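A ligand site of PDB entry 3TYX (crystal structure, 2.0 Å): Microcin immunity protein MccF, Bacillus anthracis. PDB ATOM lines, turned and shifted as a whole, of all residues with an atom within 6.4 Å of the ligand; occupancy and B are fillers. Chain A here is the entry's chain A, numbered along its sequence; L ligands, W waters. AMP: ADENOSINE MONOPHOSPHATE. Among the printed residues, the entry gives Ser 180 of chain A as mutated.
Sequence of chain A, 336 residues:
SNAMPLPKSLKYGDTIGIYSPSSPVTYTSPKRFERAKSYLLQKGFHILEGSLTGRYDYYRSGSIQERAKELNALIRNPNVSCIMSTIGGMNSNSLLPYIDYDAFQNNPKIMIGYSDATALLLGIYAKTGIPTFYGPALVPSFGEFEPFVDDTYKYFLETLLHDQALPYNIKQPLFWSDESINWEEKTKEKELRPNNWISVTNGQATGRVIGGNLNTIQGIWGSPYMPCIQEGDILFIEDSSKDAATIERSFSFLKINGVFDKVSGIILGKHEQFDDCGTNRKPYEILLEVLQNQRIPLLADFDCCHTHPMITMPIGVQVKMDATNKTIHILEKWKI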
ATOM      1  N   SER A  23      21.285 -13.537  24.339  1.00  0.00           N
ATOM      2  CA  SER A  23      20.217 -14.478  24.023  1.00  0.00           C
ATOM      3  C   SER A  23      20.707 -15.501  22.984  1.00  0.00           C
ATOM      4  O   SER A  23      21.484 -15.129  22.113  1.00  0.00           O
ATOM      5  CB  SER A  23      18.993 -13.761  23.427  1.00  0.00           C
ATOM      6  OG  SER A  23      18.503 -12.744  24.283  1.00  0.00           O
ATOM      7  N   VAL A  25      19.870 -16.885  20.215  1.00  0.00           N
ATOM      8  CA  VAL A  25      19.122 -16.794  18.968  1.00  0.00           C
ATOM      9  C   VAL A  25      19.575 -17.850  17.941  1.00  0.00           C
ATOM     10  O   VAL A  25      18.749 -18.254  17.149  1.00  0.00           O
ATOM     11  CB  VAL A  25      19.189 -15.358  18.382  1.00  0.00           C
ATOM     12  CG1 VAL A  25      20.515 -15.085  17.717  1.00  0.00           C
ATOM     13  CG2 VAL A  25      18.035 -15.065  17.437  1.00  0.00           C
ATOM     14  N   SER A  29      16.041 -19.251  16.947  1.00  0.00           N
ATOM     15  CA  SER A  29      15.565 -18.781  15.620  1.00  0.00           C
ATOM     16  C   SER A  29      16.452 -19.275  14.513  1.00  0.00           C
ATOM     17  O   SER A  29      17.220 -18.497  13.927  1.00  0.00           O
ATOM     18  CB  SER A  29      15.507 -17.264  15.625  1.00  0.00           C
ATOM     19  OG  SER A  29      14.497 -16.897  16.548  1.00  0.00           O
ATOM     20  N   ARG A  32      15.866 -17.752  10.681  1.00  0.00           N
ATOM     21  CA  ARG A  32      16.394 -16.401  10.491  1.00  0.00           C
ATOM     22  C   ARG A  32      17.921 -16.434  10.471  1.00  0.00           C
ATOM     23  O   ARG A  32      18.522 -15.831   9.586  1.00  0.00           O
ATOM     24  CB  ARG A  32      15.845 -15.412  11.502  1.00  0.00           C
ATOM     25  CG  ARG A  32      16.136 -13.981  11.066  1.00  0.00           C
ATOM     26  CD  ARG A  32      15.218 -13.068  11.783  1.00  0.00           C
ATOM     27  NE  ARG A  32      15.365 -11.676  11.486  1.00  0.00           N
ATOM     28  CZ  ARG A  32      14.410 -10.933  10.990  1.00  0.00           C
ATOM     29  NH1 ARG A  32      14.566  -9.619  10.860  1.00  0.00           N
ATOM     30  NH2 ARG A  32      13.247 -11.484  10.712  1.00  0.00           N
ATOM     31  N   ILE A  87      22.629 -11.392  18.255  1.00  0.00           N
ATOM     32  CA  ILE A  87      21.497 -10.626  18.706  1.00  0.00           C
ATOM     33  C   ILE A  87      21.874 -10.090  20.106  1.00  0.00           C
ATOM     34  O   ILE A  87      22.938 -10.460  20.646  1.00  0.00           O
ATOM     35  CB  ILE A  87      20.269 -11.538  18.785  1.00  0.00           C
ATOM     36  CG1 ILE A  87      18.979 -10.706  18.808  1.00  0.00           C
ATOM     37  CG2 ILE A  87      20.369 -12.458  19.999  1.00  0.00           C
ATOM     38  CD1 ILE A  87      17.793 -11.546  18.440  1.00  0.00           C
ATOM     39  N   GLY A  88      20.989  -9.297  20.694  1.00  0.00           N
ATOM     40  CA  GLY A  88      21.201  -8.720  22.002  1.00  0.00           C
ATOM     41  C   GLY A  88      20.526  -9.556  23.063  1.00  0.00           C
ATOM     42  O   GLY A  88      20.660 -10.766  23.066  1.00  0.00           O
ATOM     43  N   GLY A  89      19.820  -8.913  23.985  1.00  0.00           N
ATOM     44  CA  GLY A  89      19.363  -9.595  25.178  1.00  0.00           C
ATOM     45  C   GLY A  89      19.480  -8.677  26.368  1.00  0.00           C
ATOM     46  O   GLY A  89      19.069  -7.534  26.297  1.00  0.00           O
ATOM     47  N   MET A  90      19.951  -9.208  27.488  1.00  0.00           N
ATOM     48  CA  MET A  90      20.227  -8.428  28.680  1.00  0.00           C
ATOM     49  C   MET A  90      21.649  -8.496  29.212  1.00  0.00           C
ATOM     50  O   MET A  90      22.042  -7.700  30.025  1.00  0.00           O
ATOM     51  CB  MET A  90      19.327  -8.906  29.807  1.00  0.00           C
ATOM     52  CG  MET A  90      17.867  -8.600  29.617  1.00  0.00           C
ATOM     53  SD  MET A  90      17.524  -6.905  30.051  1.00  0.00           S
ATOM     54  CE  MET A  90      17.668  -6.177  28.443  1.00  0.00           C
ATOM     55  N   TYR A 114      24.070  -4.074  18.140  1.00  0.00           N
ATOM     56  CA  TYR A 114      23.255  -3.097  18.789  1.00  0.00           C
ATOM     57  C   TYR A 114      22.537  -3.596  19.992  1.00  0.00           C
ATOM     58  O   TYR A 114      22.847  -4.679  20.502  1.00  0.00           O
ATOM     59  CB  TYR A 114      22.331  -2.433  17.765  1.00  0.00           C
ATOM     60  CG  TYR A 114      21.206  -3.258  17.262  1.00  0.00           C
ATOM     61  CD1 TYR A 114      19.920  -2.979  17.631  1.00  0.00           C
ATOM     62  CD2 TYR A 114      21.420  -4.256  16.332  1.00  0.00           C
ATOM     63  CE1 TYR A 114      18.848  -3.697  17.147  1.00  0.00           C
ATOM     64  CE2 TYR A 114      20.381  -4.993  15.843  1.00  0.00           C
ATOM     65  CZ  TYR A 114      19.097  -4.730  16.251  1.00  0.00           C
ATOM     66  OH  TYR A 114      18.019  -5.449  15.743  1.00  0.00           O
ATOM     67  N   SER A 115      21.659  -2.759  20.529  1.00  0.00           N
ATOM     68  CA  SER A 115      20.825  -3.167  21.637  1.00  0.00           C
ATOM     69  C   SER A 115      21.751  -3.542  22.805  1.00  0.00           C
ATOM     70  O   SER A 115      22.759  -2.842  23.052  1.00  0.00           O
ATOM     71  CB  SER A 115      19.956  -4.355  21.166  1.00  0.00           C
ATOM     72  OG  SER A 115      18.850  -4.526  21.995  1.00  0.00           O
ATOM     73  N   ASP A 116      21.461  -4.678  23.475  1.00  0.00           N
ATOM     74  CA  ASP A 116      22.291  -5.126  24.568  1.00  0.00           C
ATOM     75  C   ASP A 116      23.789  -5.130  24.231  1.00  0.00           C
ATOM     76  O   ASP A 116      24.606  -4.965  25.137  1.00  0.00           O
ATOM     77  CB  ASP A 116      21.828  -6.514  25.043  1.00  0.00           C
ATOM     78  CG  ASP A 116      22.600  -6.994  26.309  1.00  0.00           C
ATOM     79  OD1 ASP A 116      22.468  -6.348  27.362  1.00  0.00           O
ATOM     80  OD2 ASP A 116      23.380  -8.000  26.197  1.00  0.00           O
ATOM     81  N   ALA A 117      24.167  -5.338  22.947  1.00  0.00           N
ATOM     82  CA  ALA A 117      25.585  -5.341  22.596  1.00  0.00           C
ATOM     83  C   ALA A 117      26.276  -3.953  22.889  1.00  0.00           C
ATOM     84  O   ALA A 117      27.523  -3.906  22.884  1.00  0.00           O
ATOM     85  CB  ALA A 117      25.834  -5.761  21.141  1.00  0.00           C
ATOM     86  N   ALA A 137      23.195  -6.431  13.885  1.00  0.00           N
ATOM     87  CA  ALA A 137      23.506  -7.681  14.515  1.00  0.00           C
ATOM     88  C   ALA A 137      23.056  -8.785  13.532  1.00  0.00           C
ATOM     89  O   ALA A 137      22.084  -8.617  12.856  1.00  0.00           O
ATOM     90  CB  ALA A 137      22.816  -7.876  15.841  1.00  0.00           C
ATOM     91  N   PRO A 140      18.831 -10.376  13.629  1.00  0.00           N
ATOM     92  CA  PRO A 140      17.758  -9.438  13.363  1.00  0.00           C
ATOM     93  C   PRO A 140      18.012  -8.621  12.104  1.00  0.00           C
ATOM     94  O   PRO A 140      17.083  -8.376  11.335  1.00  0.00           O
ATOM     95  CB  PRO A 140      17.704  -8.522  14.636  1.00  0.00           C
ATOM     96  CG  PRO A 140      18.985  -8.774  15.378  1.00  0.00           C
ATOM     97  CD  PRO A 140      19.519 -10.115  14.917  1.00  0.00           C
ATOM     98  N   GLU A 179       7.272  -3.393  12.214  1.00  0.00           N
ATOM     99  CA  GLU A 179       6.271  -4.499  12.341  1.00  0.00           C
ATOM    100  C   GLU A 179       6.916  -5.781  12.823  1.00  0.00           C
ATOM    101  O   GLU A 179       8.046  -6.029  12.483  1.00  0.00           O
ATOM    102  CB  GLU A 179       5.649  -4.776  10.995  1.00  0.00           C
ATOM    103  CG  GLU A 179       4.691  -3.722  10.523  1.00  0.00           C
ATOM    104  CD  GLU A 179       4.276  -3.952   9.078  1.00  0.00           C
ATOM    105  OE1 GLU A 179       4.815  -3.280   8.197  1.00  0.00           O
ATOM    106  OE2 GLU A 179       3.413  -4.788   8.816  1.00  0.00           O
ATOM    107  N   SER A 180       6.187  -6.613  13.545  1.00  0.00           N
ATOM    108  CA  SER A 180       6.767  -7.799  14.188  1.00  0.00           C
ATOM    109  C   SER A 180       6.533  -9.110  13.428  1.00  0.00           C
ATOM    110  O   SER A 180       6.919 -10.175  13.896  1.00  0.00           O
ATOM    111  CB  SER A 180       6.302  -7.958  15.653  1.00  0.00           C
ATOM    112  OG  SER A 180       4.993  -7.472  15.851  1.00  0.00           O
ATOM    113  N   ILE A 181       5.945  -9.029  12.243  1.00  0.00           N
ATOM    114  CA  ILE A 181       5.838 -10.159  11.365  1.00  0.00           C
ATOM    115  C   ILE A 181       7.186 -10.555  10.789  1.00  0.00           C
ATOM    116  O   ILE A 181       8.194  -9.857  10.960  1.00  0.00           O
ATOM    117  CB  ILE A 181       4.840  -9.864  10.243  1.00  0.00           C
ATOM    118  CG1 ILE A 181       5.385  -8.763   9.351  1.00  0.00           C
ATOM    119  CG2 ILE A 181       3.478  -9.423  10.853  1.00  0.00           C
ATOM    120  CD1 ILE A 181       4.599  -8.494   8.092  1.00  0.00           C
ATOM    121  N   ASN A 182       7.186 -11.679  10.078  1.00  0.00           N
ATOM    122  CA  ASN A 182       8.303 -12.121   9.220  1.00  0.00           C
ATOM    123  C   ASN A 182       9.610 -12.352   9.924  1.00  0.00           C
ATOM    124  O   ASN A 182      10.660 -12.056   9.369  1.00  0.00           O
ATOM    125  CB  ASN A 182       8.538 -11.193   8.018  1.00  0.00           C
ATOM    126  CG  ASN A 182       7.282 -11.006   7.198  1.00  0.00           C
ATOM    127  OD1 ASN A 182       6.300 -11.679   7.436  1.00  0.00           O
ATOM    128  ND2 ASN A 182       7.294 -10.066   6.278  1.00  0.00           N
ATOM    129  N   TRP A 183       9.523 -12.889  11.148  1.00  0.00           N
ATOM    130  CA  TRP A 183      10.672 -13.286  11.915  1.00  0.00           C
ATOM    131  C   TRP A 183      11.347 -14.531  11.390  1.00  0.00           C
ATOM    132  O   TRP A 183      12.459 -14.427  10.878  1.00  0.00           O
ATOM    133  CB  TRP A 183      10.320 -13.395  13.373  1.00  0.00           C
ATOM    134  CG  TRP A 183      11.526 -13.621  14.223  1.00  0.00           C
ATOM    135  CD1 TRP A 183      11.822 -14.738  14.956  1.00  0.00           C
ATOM    136  CD2 TRP A 183      12.676 -12.740  14.400  1.00  0.00           C
ATOM    137  NE1 TRP A 183      13.037 -14.603  15.569  1.00  0.00           N
ATOM    138  CE2 TRP A 183      13.589 -13.436  15.283  1.00  0.00           C
ATOM    139  CE3 TRP A 183      12.994 -11.430  13.980  1.00  0.00           C
ATOM    140  CZ2 TRP A 183      14.777 -12.854  15.719  1.00  0.00           C
ATOM    141  CZ3 TRP A 183      14.208 -10.876  14.392  1.00  0.00           C
ATOM    142  CH2 TRP A 183      15.069 -11.556  15.257  1.00  0.00           C
ATOM    143  N   ASN A 213      22.089   2.014  23.053  1.00  0.00           N
ATOM    144  CA  ASN A 213      20.833   1.575  23.642  1.00  0.00           C
ATOM    145  C   ASN A 213      20.745   2.062  25.063  1.00  0.00           C
ATOM    146  O   ASN A 213      21.618   1.690  25.939  1.00  0.00           O
ATOM    147  CB  ASN A 213      20.768   0.066  23.602  1.00  0.00           C
ATOM    148  CG  ASN A 213      19.426  -0.419  24.026  1.00  0.00           C
ATOM    149  OD1 ASN A 213      19.248  -0.765  25.191  1.00  0.00           O
ATOM    150  ND2 ASN A 213      18.471  -0.326  23.129  1.00  0.00           N
ATOM    151  N   SER A 240      13.976   0.223  22.505  1.00  0.00           N
ATOM    152  CA  SER A 240      12.997  -0.583  21.842  1.00  0.00           C
ATOM    153  C   SER A 240      12.037  -1.309  22.764  1.00  0.00           C
ATOM    154  O   SER A 240      12.403  -1.689  23.865  1.00  0.00           O
ATOM    155  CB  SER A 240      13.741  -1.612  20.985  1.00  0.00           C
ATOM    156  OG  SER A 240      12.781  -2.602  20.668  1.00  0.00           O
ATOM    157  N   SER A 241      10.791  -1.382  22.346  1.00  0.00           N
ATOM    158  CA  SER A 241       9.776  -2.218  22.973  1.00  0.00           C
ATOM    159  C   SER A 241       9.583  -1.915  24.445  1.00  0.00           C
ATOM    160  O   SER A 241       9.340  -2.812  25.229  1.00  0.00           O
ATOM    161  CB  SER A 241      10.097  -3.689  22.748  1.00  0.00           C
ATOM    162  OG  SER A 241      10.284  -3.955  21.383  1.00  0.00           O
ATOM    163  N   GLU A 272      11.006   1.154  18.307  1.00  0.00           N
ATOM    164  CA  GLU A 272      10.256  -0.018  17.876  1.00  0.00           C
ATOM    165  C   GLU A 272       9.178  -0.391  18.835  1.00  0.00           C
ATOM    166  O   GLU A 272       9.461  -0.659  19.996  1.00  0.00           O
ATOM    167  CB  GLU A 272      11.174  -1.199  17.718  1.00  0.00           C
ATOM    168  CG  GLU A 272      10.437  -2.488  17.317  1.00  0.00           C
ATOM    169  CD  GLU A 272      11.357  -3.675  17.365  1.00  0.00           C
ATOM    170  OE1 GLU A 272      12.104  -3.809  18.375  1.00  0.00           O
ATOM    171  OE2 GLU A 272      11.331  -4.484  16.404  1.00  0.00           O
ATOM    172  N   HIS A 306      16.130  -0.400  16.582  1.00  0.00           N
ATOM    173  CA  HIS A 306      15.499  -1.678  16.238  1.00  0.00           C
ATOM    174  C   HIS A 306      14.590  -1.694  15.035  1.00  0.00           C
ATOM    175  O   HIS A 306      14.158  -2.756  14.554  1.00  0.00           O
ATOM    176  CB  HIS A 306      14.752  -2.211  17.430  1.00  0.00           C
ATOM    177  CG  HIS A 306      15.657  -2.552  18.582  1.00  0.00           C
ATOM    178  ND1 HIS A 306      16.424  -1.598  19.211  1.00  0.00           N
ATOM    179  CD2 HIS A 306      15.874  -3.754  19.231  1.00  0.00           C
ATOM    180  CE1 HIS A 306      17.120  -2.193  20.205  1.00  0.00           C
ATOM    181  NE2 HIS A 306      16.799  -3.547  20.187  1.00  0.00           N
ATOM    182  N   HIS A 308      13.489  -1.198  11.049  1.00  0.00           N
ATOM    183  CA  HIS A 308      14.111  -1.527   9.797  1.00  0.00           C
ATOM    184  C   HIS A 308      13.846  -0.479   8.779  1.00  0.00           C
ATOM    185  O   HIS A 308      12.744  -0.038   8.654  1.00  0.00           O
ATOM    186  CB  HIS A 308      13.610  -2.857   9.290  1.00  0.00           C
ATOM    187  CG  HIS A 308      14.083  -4.000  10.093  1.00  0.00           C
ATOM    188  ND1 HIS A 308      15.309  -4.465   9.997  1.00  0.00           N
ATOM    189  CD2 HIS A 308      13.473  -4.722  11.061  1.00  0.00           C
ATOM    190  CE1 HIS A 308      15.462  -5.456  10.842  1.00  0.00           C
ATOM    191  NE2 HIS A 308      14.351  -5.602  11.505  1.00  0.00           N
HETATM  192  P   AMP L   1      17.460  -7.433  21.003  1.00  0.00           P
HETATM  193  O1P AMP L   1      16.822  -6.074  21.371  1.00  0.00           O
HETATM  194  O2P AMP L   1      17.331  -8.401  22.152  1.00  0.00           O
HETATM  195  O3P AMP L   1      18.801  -7.376  20.349  1.00  0.00           O
HETATM  196  O5' AMP L   1      16.429  -8.159  19.998  1.00  0.00           O
HETATM  197  C5' AMP L   1      16.565  -7.917  18.645  1.00  0.00           C
HETATM  198  C4' AMP L   1      15.245  -7.689  17.987  1.00  0.00           C
HETATM  199  O4' AMP L   1      14.889  -8.906  17.309  1.00  0.00           O
HETATM  200  C3' AMP L   1      14.015  -7.425  18.793  1.00  0.00           C
HETATM  201  O3' AMP L   1      13.839  -6.088  19.157  1.00  0.00           O
HETATM  202  C2' AMP L   1      13.000  -7.660  17.711  1.00  0.00           C
HETATM  203  O2' AMP L   1      13.199  -6.592  16.708  1.00  0.00           O
HETATM  204  C1' AMP L   1      13.489  -8.869  16.994  1.00  0.00           C
HETATM  205  N9  AMP L   1      12.926 -10.137  17.479  1.00  0.00           N
HETATM  206  C8  AMP L   1      13.523 -10.993  18.303  1.00  0.00           C
HETATM  207  N7  AMP L   1      12.748 -12.080  18.484  1.00  0.00           N
HETATM  208  C5  AMP L   1      11.641 -11.887  17.741  1.00  0.00           C
HETATM  209  C6  AMP L   1      10.417 -12.627  17.488  1.00  0.00           C
HETATM  210  N6  AMP L   1      10.258 -13.815  18.090  1.00  0.00           N
HETATM  211  N1  AMP L   1       9.464 -12.077  16.690  1.00  0.00           N
HETATM  212  C2  AMP L   1       9.654 -10.898  16.079  1.00  0.00           C
HETATM  213  N3  AMP L   1      10.768 -10.148  16.250  1.00  0.00           N
HETATM  214  C4  AMP L   1      11.755 -10.601  17.077  1.00  0.00           C
HETATM  215  O   HOH W   1      20.414  -7.156  18.239  1.00  0.00           O
HETATM  216  O   HOH W   2      15.460  -4.956  15.774  1.00  0.00           O
HETATM  217  O   HOH W   3      18.769  -6.339  23.785  1.00  0.00           O
HETATM  218  O   HOH W   4      17.049 -11.237  22.406  1.00  0.00           O
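The guanidinium group of Arg 32 is in hydrogen-bond range of the backbone carbonyl oxygen of Pro 140 (2.8 Å). OG of Ser 241 sits at hydrogen-bond distance from OG of Ser 240 (2.9 Å). The side-chain hydroxyl (OG) of Ser 240 is in hydrogen-bond range of the side-chain carboxylate (OE1) of Glu 272 (2.7 Å). The side-chain hydroxyl of Ser 115 lies within hydrogen-bond range of a ring nitrogen (NE2) of His 306. The backbone carbonyl oxygen (O) of Glu 272 sits at hydrogen-bond distance from the backbone NH (N) of Ser 241. OG of Ser 29 is in hydrogen-bond range of NE1 of Trp 183, 2.9 Å away. The guanidinium group (NH2) of Arg 32 is in hydrogen-bond range of the backbone carbonyl oxygen (O) of Trp 183 (3.1 Å). The backbone carbonyl oxygen (O) of Gly 88 sits at hydrogen-bond distance from the backbone NH (N) of Ser 23 (3.1 Å).
Ile 87 touches the ligand. Pro 140 touches the ligand (CB to O4', 3.9 Å). Ser 180 touches the ligand. Trp 183 touches the ligand. OG of Ser 240 touches O3' of the ligand, 3.9 Å away. Hydrophobic or aromatic side chains within 4 Å of the ligand: Ile 87, Pro 140, Trp 183 and His 306. Of the 25 residues printed, 10 come within 4 Å of the ligand.
Water W1 bridges an oxygen (O3P) of the ligand (2.7 Å) and the backbone NH of Gly 88 (3.3 Å). Water W4 lies within hydrogen-bond range of the side-chain hydroxyl (OG) of Ser 23 and an oxygen (O2P) of the ligand. Water W2 lies within hydrogen-bond range of OH of Tyr 114 (2.6 Å), O of His 306 (2.8 Å) and O2' of the ligand (2.9 Å). Water W3 lies within hydrogen-bond range of OG of Ser 115, N of Gly 89, O2P of the ligand and N of Asp 116.
O2' of the ligand is in hydrogen-bond range of OE2 of Glu 272 (2.8 Å). NE2 of His 306 lies within hydrogen-bond range of O1P of the ligand (2.8 Å). The side-chain hydroxyl (OG) of Ser 115 lies within hydrogen-bond range of an oxygen (O1P) of the ligand, at 2.6 Å. O2P of the ligand is in hydrogen-bond range of N of Gly 89 (3.1 Å). The backbone NH (N) of Gly 88 lies within hydrogen-bond range of an oxygen (O3P) of the ligand, at 2.9 Å.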
